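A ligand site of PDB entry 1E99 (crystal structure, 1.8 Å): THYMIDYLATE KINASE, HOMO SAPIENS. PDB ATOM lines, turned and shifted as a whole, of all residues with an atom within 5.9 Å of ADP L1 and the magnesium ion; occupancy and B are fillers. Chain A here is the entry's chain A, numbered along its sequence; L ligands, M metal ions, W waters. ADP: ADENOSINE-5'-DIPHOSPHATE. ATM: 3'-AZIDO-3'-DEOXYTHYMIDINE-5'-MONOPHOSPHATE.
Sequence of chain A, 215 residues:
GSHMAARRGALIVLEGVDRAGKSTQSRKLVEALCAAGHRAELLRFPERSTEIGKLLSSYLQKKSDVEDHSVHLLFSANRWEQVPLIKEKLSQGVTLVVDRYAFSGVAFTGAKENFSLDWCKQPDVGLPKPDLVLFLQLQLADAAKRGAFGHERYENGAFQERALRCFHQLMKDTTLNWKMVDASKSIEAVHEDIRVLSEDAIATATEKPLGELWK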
ATOM      1  N   GLY A  16     -14.132 -20.560 -22.021  1.00  0.00           N
ATOM      2  CA  GLY A  16     -12.800 -20.539 -21.436  1.00  0.00           C
ATOM      3  C   GLY A  16     -12.076 -19.226 -21.699  1.00  0.00           C
ATOM      4  O   GLY A  16     -12.491 -18.452 -22.556  1.00  0.00           O
ATOM      5  N   VAL A  17     -10.980 -18.991 -20.967  1.00  0.00           N
ATOM      6  CA  VAL A  17     -10.289 -17.708 -21.147  1.00  0.00           C
ATOM      7  C   VAL A  17      -9.547 -17.623 -22.466  1.00  0.00           C
ATOM      8  O   VAL A  17      -9.406 -18.616 -23.167  1.00  0.00           O
ATOM      9  CB  VAL A  17      -9.324 -17.433 -19.976  1.00  0.00           C
ATOM     10  CG1 VAL A  17     -10.153 -17.375 -18.681  1.00  0.00           C
ATOM     11  CG2 VAL A  17      -8.256 -18.502 -19.881  1.00  0.00           C
ATOM     12  N   ASP A  18      -9.009 -16.441 -22.753  1.00  0.00           N
ATOM     13  CA  ASP A  18      -8.355 -16.240 -24.040  1.00  0.00           C
ATOM     14  C   ASP A  18      -7.176 -17.192 -24.211  1.00  0.00           C
ATOM     15  O   ASP A  18      -6.423 -17.403 -23.262  1.00  0.00           O
ATOM     16  CB  ASP A  18      -7.897 -14.779 -24.172  1.00  0.00           C
ATOM     17  CG  ASP A  18      -7.579 -14.430 -25.616  1.00  0.00           C
ATOM     18  OD1 ASP A  18      -8.127 -15.007 -26.586  1.00  0.00           O
ATOM     19  OD2 ASP A  18      -6.744 -13.548 -25.825  1.00  0.00           O
ATOM     20  N   ARG A  19      -7.096 -17.846 -25.361  1.00  0.00           N
ATOM     21  CA  ARG A  19      -6.026 -18.763 -25.680  1.00  0.00           C
ATOM     22  C   ARG A  19      -5.998 -20.011 -24.849  1.00  0.00           C
ATOM     23  O   ARG A  19      -5.019 -20.754 -24.936  1.00  0.00           O
ATOM     24  CB  ARG A  19      -4.662 -18.018 -25.606  1.00  0.00           C
ATOM     25  CG  ARG A  19      -4.585 -17.007 -26.751  1.00  0.00           C
ATOM     26  CD  ARG A  19      -3.369 -16.091 -26.615  1.00  0.00           C
ATOM     27  NE  ARG A  19      -3.542 -15.082 -25.572  1.00  0.00           N
ATOM     28  CZ  ARG A  19      -2.623 -14.223 -25.161  1.00  0.00           C
ATOM     29  NH1 ARG A  19      -1.439 -14.267 -25.760  1.00  0.00           N
ATOM     30  NH2 ARG A  19      -2.819 -13.332 -24.203  1.00  0.00           N
ATOM     31  N   ALA A  20      -7.089 -20.322 -24.144  1.00  0.00           N
ATOM     32  CA  ALA A  20      -7.059 -21.541 -23.310  1.00  0.00           C
ATOM     33  C   ALA A  20      -7.159 -22.792 -24.148  1.00  0.00           C
ATOM     34  O   ALA A  20      -6.706 -23.845 -23.686  1.00  0.00           O
ATOM     35  CB  ALA A  20      -8.198 -21.452 -22.301  1.00  0.00           C
ATOM     36  N   GLY A  21      -7.607 -22.683 -25.398  1.00  0.00           N
ATOM     37  CA  GLY A  21      -7.745 -23.806 -26.289  1.00  0.00           C
ATOM     38  C   GLY A  21      -9.184 -24.213 -26.592  1.00  0.00           C
ATOM     39  O   GLY A  21      -9.430 -25.369 -26.930  1.00  0.00           O
ATOM     40  N   LYS A  22     -10.155 -23.329 -26.542  1.00  0.00           N
ATOM     41  CA  LYS A  22     -11.535 -23.727 -26.862  1.00  0.00           C
ATOM     42  C   LYS A  22     -11.644 -24.347 -28.239  1.00  0.00           C
ATOM     43  O   LYS A  22     -12.277 -25.360 -28.474  1.00  0.00           O
ATOM     44  CB  LYS A  22     -12.451 -22.476 -26.820  1.00  0.00           C
ATOM     45  CG  LYS A  22     -12.474 -21.893 -25.387  1.00  0.00           C
ATOM     46  CD  LYS A  22     -13.262 -20.592 -25.282  1.00  0.00           C
ATOM     47  CE  LYS A  22     -12.659 -19.410 -26.012  1.00  0.00           C
ATOM     48  NZ  LYS A  22     -11.283 -19.070 -25.519  1.00  0.00           N
ATOM     49  N   SER A  23     -11.036 -23.709 -29.226  1.00  0.00           N
ATOM     50  CA  SER A  23     -11.189 -24.150 -30.617  1.00  0.00           C
ATOM     51  C   SER A  23     -10.354 -25.425 -30.869  1.00  0.00           C
ATOM     52  O   SER A  23     -10.905 -26.359 -31.444  1.00  0.00           O
ATOM     53  CB  SER A  23     -10.792 -23.101 -31.641  1.00  0.00           C
ATOM     54  OG  SER A  23     -11.556 -21.909 -31.342  1.00  0.00           O
ATOM     55  N   THR A  24      -9.133 -25.407 -30.369  1.00  0.00           N
ATOM     56  CA  THR A  24      -8.355 -26.653 -30.547  1.00  0.00           C
ATOM     57  C   THR A  24      -9.021 -27.845 -29.908  1.00  0.00           C
ATOM     58  O   THR A  24      -9.143 -28.953 -30.469  1.00  0.00           O
ATOM     59  CB  THR A  24      -6.967 -26.411 -29.894  1.00  0.00           C
ATOM     60  OG1 THR A  24      -6.258 -25.428 -30.642  1.00  0.00           O
ATOM     61  CG2 THR A  24      -6.180 -27.727 -29.895  1.00  0.00           C
ATOM     62  N   GLN A  25      -9.490 -27.665 -28.665  1.00  0.00           N
ATOM     63  CA  GLN A  25     -10.112 -28.778 -27.936  1.00  0.00           C
ATOM     64  C   GLN A  25     -11.491 -29.105 -28.519  1.00  0.00           C
ATOM     65  O   GLN A  25     -11.827 -30.320 -28.541  1.00  0.00           O
ATOM     66  CB  GLN A  25     -10.213 -28.480 -26.435  1.00  0.00           C
ATOM     67  CG  GLN A  25      -8.874 -28.303 -25.721  1.00  0.00           C
ATOM     68  CD  GLN A  25      -7.945 -29.500 -25.866  1.00  0.00           C
ATOM     69  OE1 GLN A  25      -8.409 -30.605 -26.133  1.00  0.00           O
ATOM     70  NE2 GLN A  25      -6.643 -29.322 -25.646  1.00  0.00           N
ATOM     71  N   ARG A  27     -12.234 -29.031 -31.677  1.00  0.00           N
ATOM     72  CA  ARG A  27     -11.948 -29.797 -32.878  1.00  0.00           C
ATOM     73  C   ARG A  27     -11.509 -31.214 -32.521  1.00  0.00           C
ATOM     74  O   ARG A  27     -11.973 -32.190 -33.122  1.00  0.00           O
ATOM     75  CB  ARG A  27     -10.822 -29.177 -33.761  1.00  0.00           C
ATOM     76  CG  ARG A  27     -11.255 -27.833 -34.378  1.00  0.00           C
ATOM     77  CD  ARG A  27     -10.172 -27.372 -35.351  1.00  0.00           C
ATOM     78  NE  ARG A  27      -8.876 -27.163 -34.694  1.00  0.00           N
ATOM     79  CZ  ARG A  27      -8.426 -26.030 -34.204  1.00  0.00           C
ATOM     80  NH1 ARG A  27      -9.173 -24.917 -34.245  1.00  0.00           N
ATOM     81  NH2 ARG A  27      -7.200 -25.989 -33.677  1.00  0.00           N
ATOM     82  N   ASP A  99     -18.129 -24.375 -29.757  1.00  0.00           N
ATOM     83  CA  ASP A  99     -17.059 -23.475 -29.396  1.00  0.00           C
ATOM     84  C   ASP A  99     -17.648 -22.102 -29.080  1.00  0.00           C
ATOM     85  O   ASP A  99     -17.891 -21.384 -30.032  1.00  0.00           O
ATOM     86  CB  ASP A  99     -16.108 -23.404 -30.614  1.00  0.00           C
ATOM     87  CG  ASP A  99     -14.819 -22.628 -30.420  1.00  0.00           C
ATOM     88  OD1 ASP A  99     -14.643 -21.971 -29.369  1.00  0.00           O
ATOM     89  OD2 ASP A  99     -14.008 -22.638 -31.379  1.00  0.00           O
ATOM     90  N   ARG A 100     -17.906 -21.827 -27.823  1.00  0.00           N
ATOM     91  CA  ARG A 100     -18.528 -20.646 -27.273  1.00  0.00           C
ATOM     92  C   ARG A 100     -20.072 -20.729 -27.418  1.00  0.00           C
ATOM     93  O   ARG A 100     -20.541 -21.254 -28.431  1.00  0.00           O
ATOM     94  CB  ARG A 100     -18.079 -19.307 -27.794  1.00  0.00           C
ATOM     95  CG  ARG A 100     -16.583 -19.002 -27.540  1.00  0.00           C
ATOM     96  CD  ARG A 100     -16.472 -17.537 -28.078  1.00  0.00           C
ATOM     97  NE  ARG A 100     -15.090 -17.059 -28.059  1.00  0.00           N
ATOM     98  CZ  ARG A 100     -14.460 -16.533 -27.005  1.00  0.00           C
ATOM     99  NH1 ARG A 100     -15.006 -16.375 -25.805  1.00  0.00           N
ATOM    100  NH2 ARG A 100     -13.192 -16.103 -27.149  1.00  0.00           N
ATOM    101  N   ARG A 146       1.290 -18.564 -25.248  1.00  0.00           N
ATOM    102  CA  ARG A 146       0.636 -19.215 -26.381  1.00  0.00           C
ATOM    103  C   ARG A 146       0.498 -18.315 -27.604  1.00  0.00           C
ATOM    104  O   ARG A 146       0.020 -18.763 -28.651  1.00  0.00           O
ATOM    105  CB  ARG A 146      -0.760 -19.745 -25.997  1.00  0.00           C
ATOM    106  CG  ARG A 146      -0.594 -21.021 -25.189  1.00  0.00           C
ATOM    107  CD  ARG A 146      -1.928 -21.452 -24.571  1.00  0.00           C
ATOM    108  NE  ARG A 146      -1.610 -22.465 -23.567  1.00  0.00           N
ATOM    109  CZ  ARG A 146      -2.481 -23.296 -23.034  1.00  0.00           C
ATOM    110  NH1 ARG A 146      -3.757 -23.248 -23.465  1.00  0.00           N
ATOM    111  NH2 ARG A 146      -2.034 -24.156 -22.137  1.00  0.00           N
ATOM    112  N   ALA A 183      -6.636 -26.003 -18.340  1.00  0.00           N
ATOM    113  CA  ALA A 183      -6.123 -25.930 -19.718  1.00  0.00           C
ATOM    114  C   ALA A 183      -4.650 -25.611 -19.824  1.00  0.00           C
ATOM    115  O   ALA A 183      -4.177 -25.445 -20.952  1.00  0.00           O
ATOM    116  CB  ALA A 183      -6.956 -24.911 -20.495  1.00  0.00           C
ATOM    117  N   SER A 184      -3.945 -25.614 -18.693  1.00  0.00           N
ATOM    118  CA  SER A 184      -2.520 -25.345 -18.663  1.00  0.00           C
ATOM    119  C   SER A 184      -1.708 -26.561 -19.045  1.00  0.00           C
ATOM    120  O   SER A 184      -0.487 -26.430 -19.225  1.00  0.00           O
ATOM    121  CB  SER A 184      -2.099 -24.917 -17.239  1.00  0.00           C
ATOM    122  OG  SER A 184      -2.113 -26.008 -16.327  1.00  0.00           O
ATOM    123  N   LYS A 185      -2.320 -27.735 -19.099  1.00  0.00           N
ATOM    124  CA  LYS A 185      -1.592 -28.938 -19.501  1.00  0.00           C
ATOM    125  C   LYS A 185      -1.327 -28.942 -21.010  1.00  0.00           C
ATOM    126  O   LYS A 185      -1.724 -28.037 -21.720  1.00  0.00           O
ATOM    127  CB  LYS A 185      -2.367 -30.199 -19.139  1.00  0.00           C
ATOM    128  CG  LYS A 185      -2.638 -30.418 -17.653  1.00  0.00           C
ATOM    129  CD  LYS A 185      -3.886 -31.312 -17.542  1.00  0.00           C
ATOM    130  CE  LYS A 185      -3.829 -32.234 -16.350  1.00  0.00           C
ATOM    131  NZ  LYS A 185      -5.163 -32.792 -16.021  1.00  0.00           N
ATOM    132  N   SER A 186      -0.777 -30.033 -21.494  1.00  0.00           N
ATOM    133  CA  SER A 186      -0.477 -30.209 -22.908  1.00  0.00           C
ATOM    134  C   SER A 186      -1.791 -30.336 -23.668  1.00  0.00           C
ATOM    135  O   SER A 186      -2.818 -30.638 -23.053  1.00  0.00           O
ATOM    136  CB  SER A 186       0.341 -31.474 -23.180  1.00  0.00           C
ATOM    137  OG  SER A 186      -0.448 -32.667 -22.981  1.00  0.00           O
ATOM    138  N   ILE A 187      -1.729 -30.064 -24.960  1.00  0.00           N
ATOM    139  CA  ILE A 187      -2.936 -30.212 -25.783  1.00  0.00           C
ATOM    140  C   ILE A 187      -3.529 -31.600 -25.608  1.00  0.00           C
ATOM    141  O   ILE A 187      -4.751 -31.731 -25.368  1.00  0.00           O
ATOM    142  CB  ILE A 187      -2.579 -29.897 -27.246  1.00  0.00           C
ATOM    143  CG1 ILE A 187      -2.450 -28.380 -27.426  1.00  0.00           C
ATOM    144  CG2 ILE A 187      -3.621 -30.500 -28.172  1.00  0.00           C
ATOM    145  CD1 ILE A 187      -1.993 -28.022 -28.836  1.00  0.00           C
ATOM    146  N   VAL A 190      -5.031 -32.063 -21.905  1.00  0.00           N
ATOM    147  CA  VAL A 190      -6.287 -31.316 -21.756  1.00  0.00           C
ATOM    148  C   VAL A 190      -7.384 -32.072 -22.482  1.00  0.00           C
ATOM    149  O   VAL A 190      -8.508 -32.291 -22.021  1.00  0.00           O
ATOM    150  CB  VAL A 190      -6.102 -29.882 -22.263  1.00  0.00           C
ATOM    151  CG1 VAL A 190      -7.466 -29.151 -22.228  1.00  0.00           C
ATOM    152  CG2 VAL A 190      -5.127 -29.107 -21.375  1.00  0.00           C
HETATM  153  PB  ADP L   1      -8.999 -20.320 -28.052  1.00  0.00           P
HETATM  154  O1B ADP L   1      -9.408 -20.614 -26.643  1.00  0.00           O
HETATM  155  O2B ADP L   1      -9.959 -20.813 -29.075  1.00  0.00           O
HETATM  156  O3B ADP L   1      -8.634 -18.834 -28.251  1.00  0.00           O
HETATM  157  PA  ADP L   1      -6.964 -21.910 -29.485  1.00  0.00           P
HETATM  158  O1A ADP L   1      -7.076 -21.209 -30.776  1.00  0.00           O
HETATM  159  O2A ADP L   1      -7.467 -23.318 -29.417  1.00  0.00           O
HETATM  160  O3A ADP L   1      -7.583 -21.104 -28.246  1.00  0.00           O
HETATM  161  O5' ADP L   1      -5.433 -21.961 -29.055  1.00  0.00           O
HETATM  162  C5' ADP L   1      -4.647 -20.766 -28.864  1.00  0.00           C
HETATM  163  C4' ADP L   1      -3.198 -21.117 -29.294  1.00  0.00           C
HETATM  164  O4' ADP L   1      -2.643 -21.866 -28.206  1.00  0.00           O
HETATM  165  C3' ADP L   1      -3.068 -21.948 -30.562  1.00  0.00           C
HETATM  166  O3' ADP L   1      -1.839 -21.562 -31.190  1.00  0.00           O
HETATM  167  C2' ADP L   1      -2.935 -23.382 -29.990  1.00  0.00           C
HETATM  168  O2' ADP L   1      -2.143 -24.247 -30.760  1.00  0.00           O
HETATM  169  C1' ADP L   1      -2.241 -23.129 -28.637  1.00  0.00           C
HETATM  170  N9  ADP L   1      -2.687 -24.097 -27.601  1.00  0.00           N
HETATM  171  C8  ADP L   1      -3.973 -24.524 -27.410  1.00  0.00           C
HETATM  172  N7  ADP L   1      -4.076 -25.345 -26.369  1.00  0.00           N
HETATM  173  C5  ADP L   1      -2.758 -25.417 -25.858  1.00  0.00           C
HETATM  174  C6  ADP L   1      -2.255 -26.136 -24.771  1.00  0.00           C
HETATM  175  N6  ADP L   1      -2.957 -26.882 -23.984  1.00  0.00           N
HETATM  176  N1  ADP L   1      -0.947 -25.935 -24.614  1.00  0.00           N
HETATM  177  C2  ADP L   1      -0.150 -25.170 -25.374  1.00  0.00           C
HETATM  178  N3  ADP L   1      -0.573 -24.465 -26.427  1.00  0.00           N
HETATM  179  C4  ADP L   1      -1.889 -24.654 -26.570  1.00  0.00           C
HETATM  180  P   ATM L   2     -13.515 -16.483 -30.886  1.00  0.00           P
HETATM  181  OP1 ATM L   2     -12.485 -16.000 -29.869  1.00  0.00           O
HETATM  182  OP2 ATM L   2     -14.231 -17.712 -30.500  1.00  0.00           O
HETATM  183  OP3 ATM L   2     -12.855 -16.346 -32.230  1.00  0.00           O
HETATM  184  O5' ATM L   2     -14.721 -15.370 -30.793  1.00  0.00           O
HETATM  185  C5' ATM L   2     -14.555 -14.043 -31.225  1.00  0.00           C
HETATM  186  C4' ATM L   2     -15.238 -13.022 -30.275  1.00  0.00           C
HETATM  187  O4' ATM L   2     -16.637 -12.953 -30.064  1.00  0.00           O
HETATM  188  C3' ATM L   2     -14.595 -13.150 -28.914  1.00  0.00           C
HETATM  189  N3' ATM L   2     -13.884 -11.851 -28.657  1.00  0.00           N
HETATM  190  N4' ATM L   2     -12.977 -11.962 -27.811  1.00  0.00           N
HETATM  191  N5' ATM L   2     -11.972 -11.959 -27.281  1.00  0.00           N
HETATM  192  C2' ATM L   2     -15.796 -13.402 -27.956  1.00  0.00           C
HETATM  193  C1' ATM L   2     -16.947 -12.721 -28.723  1.00  0.00           C
HETATM  194  N1  ATM L   2     -18.349 -13.048 -28.443  1.00  0.00           N
HETATM  195  C2  ATM L   2     -19.226 -12.025 -28.040  1.00  0.00           C
HETATM  196  O2  ATM L   2     -18.850 -10.885 -27.771  1.00  0.00           O
HETATM  197  N3  ATM L   2     -20.533 -12.430 -27.929  1.00  0.00           N
HETATM  198  C4  ATM L   2     -20.952 -13.714 -28.211  1.00  0.00           C
HETATM  199  O4  ATM L   2     -22.272 -14.019 -28.081  1.00  0.00           O
HETATM  200  C5  ATM L   2     -19.981 -14.740 -28.657  1.00  0.00           C
HETATM  201  C5A ATM L   2     -20.405 -16.129 -28.965  1.00  0.00           C
HETATM  202  C6  ATM L   2     -18.669 -14.327 -28.758  1.00  0.00           C
HETATM  203 MG    MG M   1     -10.937 -20.009 -30.695  1.00  0.00          MG
HETATM  204  O   HOH W   1       1.411 -22.810 -27.634  1.00  0.00           O
HETATM  205  O   HOH W   2     -11.978 -19.208 -32.382  1.00  0.00           O
HETATM  206  O   HOH W   3      -4.135 -25.278 -32.190  1.00  0.00           O
HETATM  207  O   HOH W   4      -5.600 -19.943 -32.818  1.00  0.00           O
HETATM  208  O   HOH W   5       0.996 -20.847 -29.534  1.00  0.00           O
HETATM  209  O   HOH W   6      -6.743 -17.587 -29.527  1.00  0.00           O
HETATM  210  O   HOH W   7      -2.667 -19.690 -32.918  1.00  0.00           O
HETATM  211  O   HOH W   8     -10.613 -18.015 -30.157  1.00  0.00           O
HETATM  212  O   HOH W   9     -10.141 -16.981 -26.747  1.00  0.00           O
HETATM  213  O   HOH W  10       0.331 -25.437 -30.083  1.00  0.00           O
HETATM  214  O   HOH W  11      -5.803 -26.654 -24.719  1.00  0.00           O
HETATM  215  O   HOH W  12      -9.272 -20.005 -31.912  1.00  0.00           O
HETATM  216  O   HOH W  13     -12.914 -19.917 -29.660  1.00  0.00           O
HETATM  217  O   HOH W  14       0.477 -26.098 -22.421  1.00  0.00           O
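NZ of Lys 22 lies within hydrogen-bond range of O of Gly 16 (3.3 Å). The guanidinium group (NH2) of Arg 27 sits at hydrogen-bond distance from the side-chain hydroxyl (OG1) of Thr 24 (3.2 Å). The guanidinium group of Arg 19 lies within salt-bridge range of the side-chain carboxylate of Asp 18 (3.6 Å). NZ of Lys 22 lies within hydrogen-bond range of O of Val 17. The guanidinium group (NH1) of Arg 146 lies within hydrogen-bond range of the backbone carbonyl oxygen (O) of Ala 20 (3.0 Å). The backbone carbonyl oxygen (O) of Arg 19 lies within hydrogen-bond range of the guanidinium group (NH1) of Arg 146 (3.2 Å). OD2 of Asp 99 lies close to OG of Ser 23 (2.6 Å). NH2 of Arg 146 lies within hydrogen-bond range of O of Ala 183 (2.8 Å).
O of Ala 183 touches N6 of ADP L1, 3.6 Å away. C of Ser 186 touches N6 of ADP L1, at 3.7 Å. Ile 187 touches ADP L1. Hydrophobic or aromatic side chains within 4 Å of ADP L1: Ile 187. 11 residues have an atom within 4 Å of ADP L1: Arg 19, Ala 20, Gly 21, Lys 22, Ser 23, Thr 24, Arg 146, Ala 183, Lys 185, Ser 186 and Ile 187. The nearest printed residue that does not touch ADP L1 is Val 17 (4.01 Å).
The side-chain hydroxyl (OG1) of Thr 24 sits at hydrogen-bond distance from an oxygen (O2A) of ADP L1, at 2.7 Å. The backbone NH (N) of Ser 23 sits close to an oxygen (O2B) of ADP L1 (3.1 Å). The backbone NH of Arg 19 lies within hydrogen-bond range of an oxygen (O3B) of ADP L1 (3.4 Å). The backbone NH (N) of Thr 24 sits at hydrogen-bond distance from an oxygen (O2A) of ADP L1. OP2 of ATM L2 is in salt-bridge range of NE of Arg 100, at 2.7 Å. N of Lys 22 is in hydrogen-bond range of O1B of ADP L1 (2.8 Å). The backbone NH (N) of Ala 20 lies within hydrogen-bond range of an oxygen (O1B) of ADP L1, at 3.4 Å. NH2 of Arg 146 is in hydrogen-bond range of N1 of ADP L1, 3.2 Å away. NZ of Lys 22 is in salt-bridge range of O1B of ADP L1 (2.7 Å). O1B of ADP L1 sits at hydrogen-bond distance from N of Gly 21 (3.0 Å). N6 of ADP L1 lies within hydrogen-bond range of O of Lys 185 (2.8 Å).
The magnesium ion is bound by an oxygen (O2B) of ADP L1 (2.1 Å), water W12 (2.1 Å), water W8 (2.1 Å), the side-chain hydroxyl (OG) of Ser 23 (2.1 Å), water W2 (2.1 Å) and water W13 (2.2 Å).
Water W13 bridges OD1 of Asp 99 (2.7 Å) and OP2 of ATM L2 (2.7 Å). Water W8 lies within hydrogen-bond range of OP1 of ATM L2 (2.8 Å) and O3B of ADP L1 (2.9 Å). Water W3 lies within hydrogen-bond range of OG1 of Thr 24, O2' of ADP L1 and NH2 of Arg 27. Water W11 lies within hydrogen-bond range of N7 of ADP L1 (2.7 Å), NE2 of Gln 25 (2.9 Å) and O of Ala 20 (3.1 Å). Water W5 lies within hydrogen-bond range of O of Arg 146 (2.5 Å) and O3' of ADP L1 (3.4 Å).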
